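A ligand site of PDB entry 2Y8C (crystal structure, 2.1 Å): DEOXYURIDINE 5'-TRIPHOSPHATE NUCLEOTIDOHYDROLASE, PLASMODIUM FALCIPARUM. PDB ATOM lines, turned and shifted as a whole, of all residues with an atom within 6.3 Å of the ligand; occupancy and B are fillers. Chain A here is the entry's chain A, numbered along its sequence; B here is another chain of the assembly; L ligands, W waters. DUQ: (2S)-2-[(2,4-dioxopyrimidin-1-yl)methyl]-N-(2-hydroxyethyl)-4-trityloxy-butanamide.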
ATOM      1  N   PHE A  46      16.921  12.721 -20.964  1.00  0.00           N
ATOM      2  CA  PHE A  46      16.159  11.526 -20.594  1.00  0.00           C
ATOM      3  C   PHE A  46      15.327  11.968 -19.384  1.00  0.00           C
ATOM      4  O   PHE A  46      15.858  12.099 -18.294  1.00  0.00           O
ATOM      5  CB  PHE A  46      17.101  10.309 -20.356  1.00  0.00           C
ATOM      6  CG  PHE A  46      17.753   9.844 -21.612  1.00  0.00           C
ATOM      7  CD1 PHE A  46      17.036   9.100 -22.531  1.00  0.00           C
ATOM      8  CD2 PHE A  46      19.080  10.201 -21.904  1.00  0.00           C
ATOM      9  CE1 PHE A  46      17.618   8.713 -23.733  1.00  0.00           C
ATOM     10  CE2 PHE A  46      19.670   9.833 -23.100  1.00  0.00           C
ATOM     11  CZ  PHE A  46      18.953   9.090 -24.019  1.00  0.00           C
ATOM     12  N   LEU A  88       4.598   4.522 -26.092  1.00  0.00           N
ATOM     13  CA  LEU A  88       4.690   5.836 -25.507  1.00  0.00           C
ATOM     14  C   LEU A  88       4.676   6.833 -26.701  1.00  0.00           C
ATOM     15  O   LEU A  88       5.646   6.894 -27.420  1.00  0.00           O
ATOM     16  CB  LEU A  88       5.979   6.004 -24.689  1.00  0.00           C
ATOM     17  CG  LEU A  88       6.310   7.433 -24.216  1.00  0.00           C
ATOM     18  CD1 LEU A  88       5.295   7.828 -23.172  1.00  0.00           C
ATOM     19  CD2 LEU A  88       7.656   7.615 -23.560  1.00  0.00           C
ATOM     20  N   LEU A 101      10.318  13.452 -29.854  1.00  0.00           N
ATOM     21  CA  LEU A 101      10.580  12.235 -29.104  1.00  0.00           C
ATOM     22  C   LEU A 101      11.750  11.513 -29.783  1.00  0.00           C
ATOM     23  O   LEU A 101      11.634  11.066 -30.917  1.00  0.00           O
ATOM     24  CB  LEU A 101       9.326  11.324 -28.987  1.00  0.00           C
ATOM     25  CG  LEU A 101       9.407  10.290 -27.848  1.00  0.00           C
ATOM     26  CD1 LEU A 101       9.481  10.894 -26.438  1.00  0.00           C
ATOM     27  CD2 LEU A 101       8.212   9.327 -27.863  1.00  0.00           C
ATOM     28  N   ASN A 103      13.091   8.638 -29.839  1.00  0.00           N
ATOM     29  CA  ASN A 103      12.969   7.263 -30.377  1.00  0.00           C
ATOM     30  C   ASN A 103      11.721   7.063 -31.162  1.00  0.00           C
ATOM     31  O   ASN A 103      11.334   5.908 -31.375  1.00  0.00           O
ATOM     32  CB  ASN A 103      13.096   6.157 -29.297  1.00  0.00           C
ATOM     33  CG  ASN A 103      12.253   6.418 -28.031  1.00  0.00           C
ATOM     34  OD1 ASN A 103      11.965   7.610 -27.648  1.00  0.00           O
ATOM     35  ND2 ASN A 103      11.810   5.300 -27.374  1.00  0.00           N
ATOM     36  N   ILE A 105       8.416   6.648 -31.427  1.00  0.00           N
ATOM     37  CA  ILE A 105       7.428   6.059 -30.513  1.00  0.00           C
ATOM     38  C   ILE A 105       8.137   5.120 -29.536  1.00  0.00           C
ATOM     39  O   ILE A 105       8.994   4.301 -29.920  1.00  0.00           O
ATOM     40  CB  ILE A 105       6.413   5.252 -31.324  1.00  0.00           C
ATOM     41  CG1 ILE A 105       5.773   6.161 -32.398  1.00  0.00           C
ATOM     42  CG2 ILE A 105       5.354   4.717 -30.341  1.00  0.00           C
ATOM     43  CD1 ILE A 105       4.962   7.304 -31.709  1.00  0.00           C
ATOM     44  N   GLY A 106       7.891   5.272 -28.252  1.00  0.00           N
ATOM     45  CA  GLY A 106       8.597   4.410 -27.313  1.00  0.00           C
ATOM     46  C   GLY A 106       7.893   3.043 -27.227  1.00  0.00           C
ATOM     47  O   GLY A 106       6.639   2.966 -27.177  1.00  0.00           O
ATOM     48  N   LEU A 107       8.677   1.969 -27.142  1.00  0.00           N
ATOM     49  CA  LEU A 107       8.139   0.609 -27.036  1.00  0.00           C
ATOM     50  C   LEU A 107       8.402   0.136 -25.605  1.00  0.00           C
ATOM     51  O   LEU A 107       9.558  -0.036 -25.205  1.00  0.00           O
ATOM     52  CB  LEU A 107       8.724  -0.331 -28.094  1.00  0.00           C
ATOM     53  CG  LEU A 107       8.368  -1.811 -28.038  1.00  0.00           C
ATOM     54  CD1 LEU A 107       6.872  -2.082 -28.151  1.00  0.00           C
ATOM     55  CD2 LEU A 107       9.077  -2.559 -29.156  1.00  0.00           C
ATOM     56  N   ILE A 108       7.372   0.061 -24.766  1.00  0.00           N
ATOM     57  CA  ILE A 108       7.647  -0.427 -23.385  1.00  0.00           C
ATOM     58  C   ILE A 108       7.295  -1.924 -23.328  1.00  0.00           C
ATOM     59  O   ILE A 108       6.153  -2.321 -23.649  1.00  0.00           O
ATOM     60  CB  ILE A 108       7.000   0.414 -22.261  1.00  0.00           C
ATOM     61  CG1 ILE A 108       7.591   1.871 -22.275  1.00  0.00           C
ATOM     62  CG2 ILE A 108       7.220  -0.249 -20.856  1.00  0.00           C
ATOM     63  CD1 ILE A 108       6.651   2.788 -22.952  1.00  0.00           C
ATOM     64  N   ASP A 109       8.291  -2.764 -23.071  1.00  0.00           N
ATOM     65  CA  ASP A 109       8.044  -4.258 -23.138  1.00  0.00           C
ATOM     66  C   ASP A 109       7.189  -4.734 -21.970  1.00  0.00           C
ATOM     67  O   ASP A 109       7.226  -4.147 -20.883  1.00  0.00           O
ATOM     68  CB  ASP A 109       9.361  -5.059 -23.161  1.00  0.00           C
ATOM     69  CG  ASP A 109       9.999  -5.069 -24.571  1.00  0.00           C
ATOM     70  OD1 ASP A 109       9.329  -5.503 -25.540  1.00  0.00           O
ATOM     71  OD2 ASP A 109      11.142  -4.568 -24.723  1.00  0.00           O
ATOM     72  N   TYR A 112       9.022  -4.847 -18.573  1.00  0.00           N
ATOM     73  CA  TYR A 112       9.771  -3.716 -18.060  1.00  0.00           C
ATOM     74  C   TYR A 112       9.119  -3.292 -16.710  1.00  0.00           C
ATOM     75  O   TYR A 112       7.890  -3.095 -16.593  1.00  0.00           O
ATOM     76  CB  TYR A 112       9.732  -2.545 -19.071  1.00  0.00           C
ATOM     77  CG  TYR A 112      10.507  -1.348 -18.597  1.00  0.00           C
ATOM     78  CD1 TYR A 112      11.902  -1.442 -18.407  1.00  0.00           C
ATOM     79  CD2 TYR A 112       9.882  -0.125 -18.368  1.00  0.00           C
ATOM     80  CE1 TYR A 112      12.645  -0.355 -17.977  1.00  0.00           C
ATOM     81  CE2 TYR A 112      10.639   0.978 -17.940  1.00  0.00           C
ATOM     82  CZ  TYR A 112      12.028   0.847 -17.769  1.00  0.00           C
ATOM     83  OH  TYR A 112      12.822   1.882 -17.313  1.00  0.00           O
ATOM     84  N   GLY A 114      11.095  -0.838 -14.923  1.00  0.00           N
ATOM     85  CA  GLY A 114      11.795   0.400 -14.415  1.00  0.00           C
ATOM     86  C   GLY A 114      10.908   1.637 -14.524  1.00  0.00           C
ATOM     87  O   GLY A 114       9.773   1.522 -14.982  1.00  0.00           O
ATOM     88  N   GLU A 115      11.415   2.783 -14.066  1.00  0.00           N
ATOM     89  CA  GLU A 115      10.791   4.107 -14.238  1.00  0.00           C
ATOM     90  C   GLU A 115      10.545   4.387 -15.737  1.00  0.00           C
ATOM     91  O   GLU A 115      11.435   4.134 -16.574  1.00  0.00           O
ATOM     92  CB  GLU A 115      11.636   5.185 -13.590  1.00  0.00           C
ATOM     93  CG  GLU A 115      10.847   6.498 -13.455  1.00  0.00           C
ATOM     94  CD  GLU A 115      11.522   7.540 -12.647  1.00  0.00           C
ATOM     95  OE1 GLU A 115      12.660   7.250 -12.277  1.00  0.00           O
ATOM     96  OE2 GLU A 115      10.971   8.651 -12.393  1.00  0.00           O
ATOM     97  N   ILE A 116       9.369   4.924 -16.075  1.00  0.00           N
ATOM     98  CA  ILE A 116       9.063   5.249 -17.505  1.00  0.00           C
ATOM     99  C   ILE A 116       9.837   6.585 -17.810  1.00  0.00           C
ATOM    100  O   ILE A 116       9.739   7.565 -17.062  1.00  0.00           O
ATOM    101  CB  ILE A 116       7.543   5.471 -17.737  1.00  0.00           C
ATOM    102  CG1 ILE A 116       6.791   4.132 -18.010  1.00  0.00           C
ATOM    103  CG2 ILE A 116       7.289   5.977 -19.156  1.00  0.00           C
ATOM    104  CD1 ILE A 116       6.697   3.160 -16.928  1.00  0.00           C
ATOM    105  N   ILE A 117      10.550   6.649 -18.924  1.00  0.00           N
ATOM    106  CA  ILE A 117      11.384   7.833 -19.187  1.00  0.00           C
ATOM    107  C   ILE A 117      11.048   8.371 -20.585  1.00  0.00           C
ATOM    108  O   ILE A 117      10.868   7.581 -21.511  1.00  0.00           O
ATOM    109  CB  ILE A 117      12.898   7.370 -19.167  1.00  0.00           C
ATOM    110  CG1 ILE A 117      13.315   6.978 -17.731  1.00  0.00           C
ATOM    111  CG2 ILE A 117      13.805   8.464 -19.691  1.00  0.00           C
ATOM    112  CD1 ILE A 117      14.483   6.026 -17.764  1.00  0.00           C
ATOM    113  N   ALA A 118      10.943   9.703 -20.757  1.00  0.00           N
ATOM    114  CA  ALA A 118      10.792  10.240 -22.172  1.00  0.00           C
ATOM    115  C   ALA A 118      12.117  10.798 -22.691  1.00  0.00           C
ATOM    116  O   ALA A 118      12.660  11.680 -22.079  1.00  0.00           O
ATOM    117  CB  ALA A 118       9.767  11.330 -22.179  1.00  0.00           C
ATOM    118  N   ALA A 119      12.578  10.321 -23.843  1.00  0.00           N
ATOM    119  CA  ALA A 119      13.854  10.824 -24.398  1.00  0.00           C
ATOM    120  C   ALA A 119      13.448  12.003 -25.283  1.00  0.00           C
ATOM    121  O   ALA A 119      12.953  11.792 -26.352  1.00  0.00           O
ATOM    122  CB  ALA A 119      14.505   9.717 -25.280  1.00  0.00           C
ATOM    123  N   ARG A 160      12.580  -4.210  -7.858  1.00  0.00           N
ATOM    124  CA  ARG A 160      12.383  -3.259  -8.976  1.00  0.00           C
ATOM    125  C   ARG A 160      10.864  -3.001  -9.231  1.00  0.00           C
ATOM    126  O   ARG A 160      10.477  -1.868  -9.548  1.00  0.00           O
ATOM    127  CB  ARG A 160      13.008  -3.774 -10.285  1.00  0.00           C
ATOM    128  CG  ARG A 160      13.239  -2.695 -11.362  1.00  0.00           C
ATOM    129  CD  ARG A 160      14.259  -3.136 -12.440  1.00  0.00           C
ATOM    130  NE  ARG A 160      14.811  -1.924 -13.076  1.00  0.00           N
ATOM    131  CZ  ARG A 160      14.795  -1.608 -14.384  1.00  0.00           C
ATOM    132  NH1 ARG A 160      14.331  -2.447 -15.310  1.00  0.00           N
ATOM    133  NH2 ARG A 160      15.304  -0.424 -14.759  1.00  0.00           N
ATOM    134  N   ARG B  91      15.422   1.428 -32.077  1.00  0.00           N
ATOM    135  CA  ARG B  91      15.593   0.793 -30.789  1.00  0.00           C
ATOM    136  C   ARG B  91      15.677   1.970 -29.837  1.00  0.00           C
ATOM    137  O   ARG B  91      16.204   3.034 -30.217  1.00  0.00           O
ATOM    138  CB  ARG B  91      16.911  -0.036 -30.711  1.00  0.00           C
ATOM    139  CG  ARG B  91      16.790  -1.424 -31.348  1.00  0.00           C
ATOM    140  CD  ARG B  91      18.070  -2.304 -31.194  1.00  0.00           C
ATOM    141  NE  ARG B  91      18.230  -2.912 -29.863  1.00  0.00           N
ATOM    142  CZ  ARG B  91      19.194  -2.570 -29.026  1.00  0.00           C
ATOM    143  NH1 ARG B  91      20.104  -1.671 -29.380  1.00  0.00           N
ATOM    144  NH2 ARG B  91      19.266  -3.106 -27.837  1.00  0.00           N
ATOM    145  N   SER B  92      15.224   1.742 -28.586  1.00  0.00           N
ATOM    146  CA  SER B  92      15.356   2.717 -27.540  1.00  0.00           C
ATOM    147  C   SER B  92      16.724   3.343 -27.468  1.00  0.00           C
ATOM    148  O   SER B  92      16.850   4.563 -27.232  1.00  0.00           O
ATOM    149  CB  SER B  92      15.041   2.083 -26.170  1.00  0.00           C
ATOM    150  OG  SER B  92      13.670   1.790 -26.231  1.00  0.00           O
ATOM    151  N   SER B  93      17.751   2.515 -27.576  1.00  0.00           N
ATOM    152  CA  SER B  93      19.164   3.022 -27.398  1.00  0.00           C
ATOM    153  C   SER B  93      19.609   3.965 -28.548  1.00  0.00           C
ATOM    154  O   SER B  93      20.566   4.742 -28.335  1.00  0.00           O
ATOM    155  CB  SER B  93      20.164   1.843 -27.323  1.00  0.00           C
ATOM    156  OG  SER B  93      19.989   1.011 -28.461  1.00  0.00           O
ATOM    157  N   ILE B  94      18.902   3.992 -29.676  1.00  0.00           N
ATOM    158  CA  ILE B  94      19.253   5.024 -30.742  1.00  0.00           C
ATOM    159  C   ILE B  94      19.294   6.432 -30.169  1.00  0.00           C
ATOM    160  O   ILE B  94      19.985   7.293 -30.651  1.00  0.00           O
ATOM    161  CB  ILE B  94      18.290   4.997 -31.943  1.00  0.00           C
ATOM    162  CG1 ILE B  94      19.008   5.473 -33.212  1.00  0.00           C
ATOM    163  CG2 ILE B  94      17.012   5.868 -31.699  1.00  0.00           C
ATOM    164  CD1 ILE B  94      18.367   5.021 -34.488  1.00  0.00           C
ATOM    165  N   SER B  95      18.558   6.661 -29.083  1.00  0.00           N
ATOM    166  CA  SER B  95      18.382   8.001 -28.523  1.00  0.00           C
ATOM    167  C   SER B  95      19.648   8.663 -28.066  1.00  0.00           C
ATOM    168  O   SER B  95      19.688   9.890 -27.957  1.00  0.00           O
ATOM    169  CB  SER B  95      17.426   7.941 -27.337  1.00  0.00           C
ATOM    170  OG  SER B  95      16.128   7.641 -27.859  1.00  0.00           O
ATOM    171  N   LYS B  96      20.633   7.845 -27.694  1.00  0.00           N
ATOM    172  CA  LYS B  96      21.933   8.301 -27.177  1.00  0.00           C
ATOM    173  C   LYS B  96      22.773   8.802 -28.345  1.00  0.00           C
ATOM    174  O   LYS B  96      23.742   9.529 -28.145  1.00  0.00           O
ATOM    175  CB  LYS B  96      22.700   7.088 -26.567  1.00  0.00           C
ATOM    176  CG  LYS B  96      23.415   7.440 -25.274  1.00  0.00           C
HETATM  177  O4  DUQ L   1      10.333   5.490 -24.575  1.00  0.00           O
HETATM  178  C4  DUQ L   1      10.742   4.628 -23.771  1.00  0.00           C
HETATM  179  N3  DUQ L   1      10.870   4.876 -22.433  1.00  0.00           N
HETATM  180  C2  DUQ L   1      11.323   3.900 -21.608  1.00  0.00           C
HETATM  181  O2  DUQ L   1      11.444   4.039 -20.366  1.00  0.00           O
HETATM  182  C5  DUQ L   1      11.084   3.413 -24.293  1.00  0.00           C
HETATM  183  C6  DUQ L   1      11.585   2.414 -23.437  1.00  0.00           C
HETATM  184  N1  DUQ L   1      11.680   2.648 -22.124  1.00  0.00           N
HETATM  185  C1' DUQ L   1      12.248   1.654 -21.175  1.00  0.00           C
HETATM  186  C1  DUQ L   1      13.660   1.275 -21.652  1.00  0.00           C
HETATM  187  C38 DUQ L   1      14.407   0.220 -20.846  1.00  0.00           C
HETATM  188  N34 DUQ L   1      15.266   0.493 -19.870  1.00  0.00           N
HETATM  189  C39 DUQ L   1      15.975  -0.519 -19.076  1.00  0.00           C
HETATM  190  C40 DUQ L   1      16.651   0.269 -17.955  1.00  0.00           C
HETATM  191  O37 DUQ L   1      17.813   0.892 -18.524  1.00  0.00           O
HETATM  192  O38 DUQ L   1      14.209  -0.900 -21.192  1.00  0.00           O
HETATM  193  C4' DUQ L   1      14.529   2.463 -21.976  1.00  0.00           C
HETATM  194  C5' DUQ L   1      15.978   2.177 -22.396  1.00  0.00           C
HETATM  195  O1  DUQ L   1      16.694   3.027 -21.466  1.00  0.00           O
HETATM  196  C17 DUQ L   1      17.185   4.325 -21.899  1.00  0.00           C
HETATM  197  C30 DUQ L   1      17.564   4.990 -20.590  1.00  0.00           C
HETATM  198  C31 DUQ L   1      17.676   4.208 -19.419  1.00  0.00           C
HETATM  199  C32 DUQ L   1      18.016   4.856 -18.206  1.00  0.00           C
HETATM  200  C33 DUQ L   1      18.281   6.230 -18.130  1.00  0.00           C
HETATM  201  C34 DUQ L   1      18.199   6.984 -19.317  1.00  0.00           C
HETATM  202  C35 DUQ L   1      17.876   6.352 -20.504  1.00  0.00           C
HETATM  203  C24 DUQ L   1      18.484   4.065 -22.647  1.00  0.00           C
HETATM  204  C25 DUQ L   1      19.116   2.797 -22.505  1.00  0.00           C
HETATM  205  C26 DUQ L   1      20.333   2.522 -23.174  1.00  0.00           C
HETATM  206  C27 DUQ L   1      20.936   3.531 -23.943  1.00  0.00           C
HETATM  207  C28 DUQ L   1      20.330   4.806 -24.072  1.00  0.00           C
HETATM  208  C29 DUQ L   1      19.103   5.060 -23.424  1.00  0.00           C
HETATM  209  C18 DUQ L   1      16.072   5.060 -22.703  1.00  0.00           C
HETATM  210  C19 DUQ L   1      14.958   5.642 -22.033  1.00  0.00           C
HETATM  211  C20 DUQ L   1      13.890   6.282 -22.760  1.00  0.00           C
HETATM  212  C21 DUQ L   1      13.966   6.354 -24.148  1.00  0.00           C
HETATM  213  C22 DUQ L   1      15.060   5.773 -24.846  1.00  0.00           C
HETATM  214  C23 DUQ L   1      16.088   5.129 -24.114  1.00  0.00           C
HETATM  215  O   HOH W   1      11.101   8.200 -25.097  1.00  0.00           O
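Phe 46 touches the ligand. Leu 88 touches the ligand. CA of Gly 106 touches O4 of the ligand, 3.4 Å away. O of Leu 107 touches C6 of the ligand (3.6 Å). CE1 of Tyr 112 touches N34 of the ligand, 3.3 Å away. Glu 115 touches the ligand (O to O2, 3.8 Å). Ile 116 touches the ligand (CA to O2, 3.9 Å). Ala 119 touches the ligand (CB to C21, 3.6 Å). NH2 of Arg 160 touches C40 of the ligand, at 3.5 Å. O of Ser 92 of chain B touches C22 of the ligand (3.2 Å). Ser 93 of chain B touches the ligand. Ser 95 of chain B touches the ligand (OG to C22, 3.7 Å). Of the 23 residues printed, 14 come within 4 Å of the ligand.
Water W1 lies within hydrogen-bond range of OD1 of Asn 103, O4 of the ligand and N of Ala 119.
A nitrogen (N3) of the ligand sits at hydrogen-bond distance from the backbone carbonyl oxygen of Ile 117 (2.9 Å). ND2 of Asn 103 sits at hydrogen-bond distance from O4 of the ligand (3.2 Å). An oxygen (O2) of the ligand is in hydrogen-bond range of the backbone NH (N) of Ile 117 (3.1 Å).
O of Ser 92 of chain B lies within hydrogen-bond range of OG of Ser 95 of chain B, at 3.2 Å. The guanidinium group (NH1) of Arg 91 of chain B lies within hydrogen-bond range of the side-chain hydroxyl (OG) of Ser 93 of chain B (2.8 Å). The backbone carbonyl oxygen (O) of Gly 106 sits at hydrogen-bond distance from the backbone NH (N) of Leu 88, 2.8 Å away. The backbone carbonyl oxygen (O) of Glu 115 lies within hydrogen-bond range of the side-chain hydroxyl (OH) of Tyr 112 (2.7 Å).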
